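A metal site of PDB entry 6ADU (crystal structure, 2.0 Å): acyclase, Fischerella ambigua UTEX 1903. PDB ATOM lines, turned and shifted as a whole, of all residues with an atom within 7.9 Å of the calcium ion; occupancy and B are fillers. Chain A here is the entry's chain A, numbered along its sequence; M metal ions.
Within 4 Å of the calcium ion: Gly 37, Glu 39, Glu 95, Asn 98 and Asp 216.
The nearest printed residue that does not touch the calcium ion is Gly 96 (4.4 Å).
The calcium ion is bound by O of Asn 98 (2.2 Å), OE2 of Glu 95 (2.3 Å), O of Gly 37 (2.4 Å), O of Glu 95 (2.4 Å), OE2 of Glu 39 (2.4 Å), OD1 of Asp 216 (2.4 Å) and OD2 of Asp 216 (2.7 Å).
The calcium ion has seven donor atoms within binding distance.
ND2 of Asn 98 is in hydrogen-bond range of O of Phe 38 (3.0 Å).
The backbone NH (N) of Glu 39 is in hydrogen-bond range of the side-chain amide oxygen (OD1) of Asn 35.
OE1 of Glu 39 is in hydrogen-bond range of N of Arg 97 (3.0 Å).
O of Asp 216 sits at hydrogen-bond distance from N of Asp 134 (2.9 Å).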
ATOM      1  N   ASN A  35     -11.775  22.118  18.176  1.00  0.00           N
ATOM      2  CA  ASN A  35     -12.911  21.773  17.348  1.00  0.00           C
ATOM      3  C   ASN A  35     -13.902  22.936  17.283  1.00  0.00           C
ATOM      4  O   ASN A  35     -15.108  22.735  17.358  1.00  0.00           O
ATOM      5  CB  ASN A  35     -13.540  20.478  17.824  1.00  0.00           C
ATOM      6  CG  ASN A  35     -14.446  19.812  16.810  1.00  0.00           C
ATOM      7  OD1 ASN A  35     -14.335  20.071  15.589  1.00  0.00           O
ATOM      8  ND2 ASN A  35     -15.325  18.965  17.313  1.00  0.00           N
ATOM      9  N   ALA A  36     -13.366  24.110  16.980  1.00  0.00           N
ATOM     10  CA  ALA A  36     -14.067  25.371  17.119  1.00  0.00           C
ATOM     11  C   ALA A  36     -15.089  25.544  16.005  1.00  0.00           C
ATOM     12  O   ALA A  36     -16.023  26.319  16.187  1.00  0.00           O
ATOM     13  CB  ALA A  36     -13.098  26.520  17.201  1.00  0.00           C
ATOM     14  N   GLY A  37     -14.908  24.864  14.871  1.00  0.00           N
ATOM     15  CA  GLY A  37     -15.932  24.847  13.815  1.00  0.00           C
ATOM     16  C   GLY A  37     -16.638  23.520  13.672  1.00  0.00           C
ATOM     17  O   GLY A  37     -17.250  23.257  12.671  1.00  0.00           O
ATOM     18  N   PHE A  38     -16.601  22.684  14.720  1.00  0.00           N
ATOM     19  CA  PHE A  38     -17.286  21.392  14.737  1.00  0.00           C
ATOM     20  C   PHE A  38     -16.988  20.520  13.508  1.00  0.00           C
ATOM     21  O   PHE A  38     -17.833  19.709  13.160  1.00  0.00           O
ATOM     22  CB  PHE A  38     -18.799  21.578  14.865  1.00  0.00           C
ATOM     23  CG  PHE A  38     -19.195  22.362  16.090  1.00  0.00           C
ATOM     24  CD1 PHE A  38     -19.216  21.769  17.348  1.00  0.00           C
ATOM     25  CD2 PHE A  38     -19.456  23.721  16.003  1.00  0.00           C
ATOM     26  CE1 PHE A  38     -19.538  22.510  18.486  1.00  0.00           C
ATOM     27  CE2 PHE A  38     -19.768  24.454  17.130  1.00  0.00           C
ATOM     28  CZ  PHE A  38     -19.803  23.850  18.375  1.00  0.00           C
ATOM     29  N   GLU A  39     -15.784  20.640  12.941  1.00  0.00           N
ATOM     30  CA  GLU A  39     -15.366  19.929  11.728  1.00  0.00           C
ATOM     31  C   GLU A  39     -15.057  18.459  12.045  1.00  0.00           C
ATOM     32  O   GLU A  39     -15.057  17.607  11.130  1.00  0.00           O
ATOM     33  CB  GLU A  39     -14.202  20.654  11.070  1.00  0.00           C
ATOM     34  CG  GLU A  39     -14.612  21.988  10.468  1.00  0.00           C
ATOM     35  CD  GLU A  39     -15.780  21.873   9.502  1.00  0.00           C
ATOM     36  OE1 GLU A  39     -15.677  21.077   8.541  1.00  0.00           O
ATOM     37  OE2 GLU A  39     -16.805  22.504   9.739  1.00  0.00           O
ATOM     38  N   ASP A  40     -14.832  18.155  13.343  1.00  0.00           N
ATOM     39  CA  ASP A  40     -14.735  16.753  13.820  1.00  0.00           C
ATOM     40  C   ASP A  40     -16.048  16.329  14.483  1.00  0.00           C
ATOM     41  O   ASP A  40     -16.497  17.015  15.379  1.00  0.00           O
ATOM     42  CB  ASP A  40     -13.639  16.593  14.877  1.00  0.00           C
ATOM     43  CG  ASP A  40     -12.228  16.541  14.325  1.00  0.00           C
ATOM     44  OD1 ASP A  40     -12.078  16.571  13.087  1.00  0.00           O
ATOM     45  OD2 ASP A  40     -11.310  16.360  15.135  1.00  0.00           O
ATOM     46  N   GLY A  80     -23.396  18.414  12.261  1.00  0.00           N
ATOM     47  CA  GLY A  80     -24.302  18.240  11.078  1.00  0.00           C
ATOM     48  C   GLY A  80     -23.709  18.915   9.863  1.00  0.00           C
ATOM     49  O   GLY A  80     -23.135  20.001   9.967  1.00  0.00           O
ATOM     50  N   ALA A  93     -22.590  26.000   5.637  1.00  0.00           N
ATOM     51  CA  ALA A  93     -22.069  26.246   6.952  1.00  0.00           C
ATOM     52  C   ALA A  93     -21.260  27.536   6.928  1.00  0.00           C
ATOM     53  O   ALA A  93     -20.559  27.825   5.948  1.00  0.00           O
ATOM     54  CB  ALA A  93     -21.212  25.097   7.401  1.00  0.00           C
ATOM     55  N   PRO A  94     -21.336  28.360   8.001  1.00  0.00           N
ATOM     56  CA  PRO A  94     -20.474  29.524   8.153  1.00  0.00           C
ATOM     57  C   PRO A  94     -18.982  29.243   7.954  1.00  0.00           C
ATOM     58  O   PRO A  94     -18.295  30.121   7.468  1.00  0.00           O
ATOM     59  CB  PRO A  94     -20.748  30.013   9.582  1.00  0.00           C
ATOM     60  CG  PRO A  94     -22.161  29.538   9.871  1.00  0.00           C
ATOM     61  CD  PRO A  94     -22.336  28.260   9.080  1.00  0.00           C
ATOM     62  N   GLU A  95     -18.542  28.024   8.278  1.00  0.00           N
ATOM     63  CA  GLU A  95     -17.114  27.630   8.186  1.00  0.00           C
ATOM     64  C   GLU A  95     -17.038  26.127   7.874  1.00  0.00           C
ATOM     65  O   GLU A  95     -17.726  25.343   8.482  1.00  0.00           O
ATOM     66  CB  GLU A  95     -16.456  28.041   9.502  1.00  0.00           C
ATOM     67  CG  GLU A  95     -15.047  27.531   9.741  1.00  0.00           C
ATOM     68  CD  GLU A  95     -14.892  26.065  10.114  1.00  0.00           C
ATOM     69  OE1 GLU A  95     -13.783  25.582   9.930  1.00  0.00           O
ATOM     70  OE2 GLU A  95     -15.862  25.417  10.594  1.00  0.00           O
ATOM     71  N   GLY A  96     -16.197  25.723   6.935  1.00  0.00           N
ATOM     72  CA  GLY A  96     -16.010  24.289   6.575  1.00  0.00           C
ATOM     73  C   GLY A  96     -17.314  23.627   6.173  1.00  0.00           C
ATOM     74  O   GLY A  96     -18.186  24.266   5.574  1.00  0.00           O
ATOM     75  N   ARG A  97     -17.492  22.357   6.597  1.00  0.00           N
ATOM     76  CA  ARG A  97     -18.611  21.507   6.228  1.00  0.00           C
ATOM     77  C   ARG A  97     -19.755  21.468   7.275  1.00  0.00           C
ATOM     78  O   ARG A  97     -20.920  21.328   6.940  1.00  0.00           O
ATOM     79  CB  ARG A  97     -18.086  20.068   6.088  1.00  0.00           C
ATOM     80  CG  ARG A  97     -17.039  19.848   5.009  1.00  0.00           C
ATOM     81  CD  ARG A  97     -16.477  18.416   5.046  1.00  0.00           C
ATOM     82  NE  ARG A  97     -17.470  17.402   4.721  1.00  0.00           N
ATOM     83  CZ  ARG A  97     -17.676  16.914   3.505  1.00  0.00           C
ATOM     84  NH1 ARG A  97     -17.014  17.435   2.482  1.00  0.00           N
ATOM     85  NH2 ARG A  97     -18.508  15.914   3.318  1.00  0.00           N
ATOM     86  N   ASN A  98     -19.392  21.562   8.563  1.00  0.00           N
ATOM     87  CA  ASN A  98     -20.250  21.202   9.655  1.00  0.00           C
ATOM     88  C   ASN A  98     -20.593  22.401  10.537  1.00  0.00           C
ATOM     89  O   ASN A  98     -19.827  23.389  10.628  1.00  0.00           O
ATOM     90  CB  ASN A  98     -19.599  20.200  10.609  1.00  0.00           C
ATOM     91  CG  ASN A  98     -19.288  18.854   9.999  1.00  0.00           C
ATOM     92  OD1 ASN A  98     -19.794  18.502   8.925  1.00  0.00           O
ATOM     93  ND2 ASN A  98     -18.437  18.093  10.695  1.00  0.00           N
ATOM     94  N   ILE A  99     -21.715  22.205  11.246  1.00  0.00           N
ATOM     95  CA  ILE A  99     -22.155  23.046  12.373  1.00  0.00           C
ATOM     96  C   ILE A  99     -22.361  22.127  13.596  1.00  0.00           C
ATOM     97  O   ILE A  99     -22.434  20.937  13.441  1.00  0.00           O
ATOM     98  CB  ILE A  99     -23.422  23.822  11.947  1.00  0.00           C
ATOM     99  CG1 ILE A  99     -24.628  22.939  11.596  1.00  0.00           C
ATOM    100  CG2 ILE A  99     -23.086  24.693  10.745  1.00  0.00           C
ATOM    101  CD1 ILE A  99     -25.223  22.196  12.763  1.00  0.00           C
ATOM    102  N   GLY A 100     -22.442  22.714  14.798  1.00  0.00           N
ATOM    103  CA  GLY A 100     -22.844  21.999  16.028  1.00  0.00           C
ATOM    104  C   GLY A 100     -24.276  22.366  16.311  1.00  0.00           C
ATOM    105  O   GLY A 100     -24.569  23.561  16.390  1.00  0.00           O
ATOM    106  N   ASP A 134     -21.257  32.036  15.058  1.00  0.00           N
ATOM    107  CA  ASP A 134     -22.408  32.074  14.156  1.00  0.00           C
ATOM    108  C   ASP A 134     -23.534  31.188  14.734  1.00  0.00           C
ATOM    109  O   ASP A 134     -23.298  30.120  15.277  1.00  0.00           O
ATOM    110  CB  ASP A 134     -21.982  31.696  12.743  1.00  0.00           C
ATOM    111  CG  ASP A 134     -20.789  32.535  12.291  1.00  0.00           C
ATOM    112  OD1 ASP A 134     -20.850  33.775  12.388  1.00  0.00           O
ATOM    113  OD2 ASP A 134     -19.760  31.925  11.910  1.00  0.00           O
ATOM    114  N   PHE A 215     -24.765  26.254  15.862  1.00  0.00           N
ATOM    115  CA  PHE A 215     -23.652  27.118  16.066  1.00  0.00           C
ATOM    116  C   PHE A 215     -22.475  26.726  15.173  1.00  0.00           C
ATOM    117  O   PHE A 215     -22.313  25.588  14.799  1.00  0.00           O
ATOM    118  CB  PHE A 215     -23.164  27.046  17.516  1.00  0.00           C
ATOM    119  CG  PHE A 215     -24.149  27.515  18.547  1.00  0.00           C
ATOM    120  CD1 PHE A 215     -24.270  28.851  18.849  1.00  0.00           C
ATOM    121  CD2 PHE A 215     -24.922  26.595  19.252  1.00  0.00           C
ATOM    122  CE1 PHE A 215     -25.158  29.289  19.821  1.00  0.00           C
ATOM    123  CE2 PHE A 215     -25.832  27.049  20.211  1.00  0.00           C
ATOM    124  CZ  PHE A 215     -25.937  28.389  20.498  1.00  0.00           C
ATOM    125  N   ASP A 216     -21.624  27.694  14.879  1.00  0.00           N
ATOM    126  CA  ASP A 216     -20.419  27.400  14.086  1.00  0.00           C
ATOM    127  C   ASP A 216     -19.401  28.526  14.214  1.00  0.00           C
ATOM    128  O   ASP A 216     -19.729  29.659  14.609  1.00  0.00           O
ATOM    129  CB  ASP A 216     -20.765  27.145  12.600  1.00  0.00           C
ATOM    130  CG  ASP A 216     -19.682  26.424  11.834  1.00  0.00           C
ATOM    131  OD1 ASP A 216     -18.740  25.887  12.505  1.00  0.00           O
ATOM    132  OD2 ASP A 216     -19.711  26.441  10.558  1.00  0.00           O
ATOM    133  N   ASN A 217     -18.137  28.203  13.916  1.00  0.00           N
ATOM    134  CA  ASN A 217     -17.065  29.151  13.721  1.00  0.00           C
ATOM    135  C   ASN A 217     -16.822  29.958  15.024  1.00  0.00           C
ATOM    136  O   ASN A 217     -16.755  31.158  15.000  1.00  0.00           O
ATOM    137  CB  ASN A 217     -17.322  30.074  12.513  1.00  0.00           C
ATOM    138  CG  ASN A 217     -16.071  30.798  12.051  1.00  0.00           C
ATOM    139  OD1 ASN A 217     -14.951  30.364  12.347  1.00  0.00           O
ATOM    140  ND2 ASN A 217     -16.229  31.919  11.353  1.00  0.00           N
ATOM    141  N   VAL A 218     -16.621  29.256  16.141  1.00  0.00           N
ATOM    142  CA  VAL A 218     -16.346  29.883  17.412  1.00  0.00           C
ATOM    143  C   VAL A 218     -14.925  30.465  17.352  1.00  0.00           C
ATOM    144  O   VAL A 218     -13.957  29.731  17.036  1.00  0.00           O
ATOM    145  CB  VAL A 218     -16.510  28.888  18.578  1.00  0.00           C
ATOM    146  CG1 VAL A 218     -16.359  29.527  19.934  1.00  0.00           C
ATOM    147  CG2 VAL A 218     -17.805  28.116  18.500  1.00  0.00           C
HETATM  148 CA    CA M   1     -17.941  24.428  10.708  1.00  0.00          CA
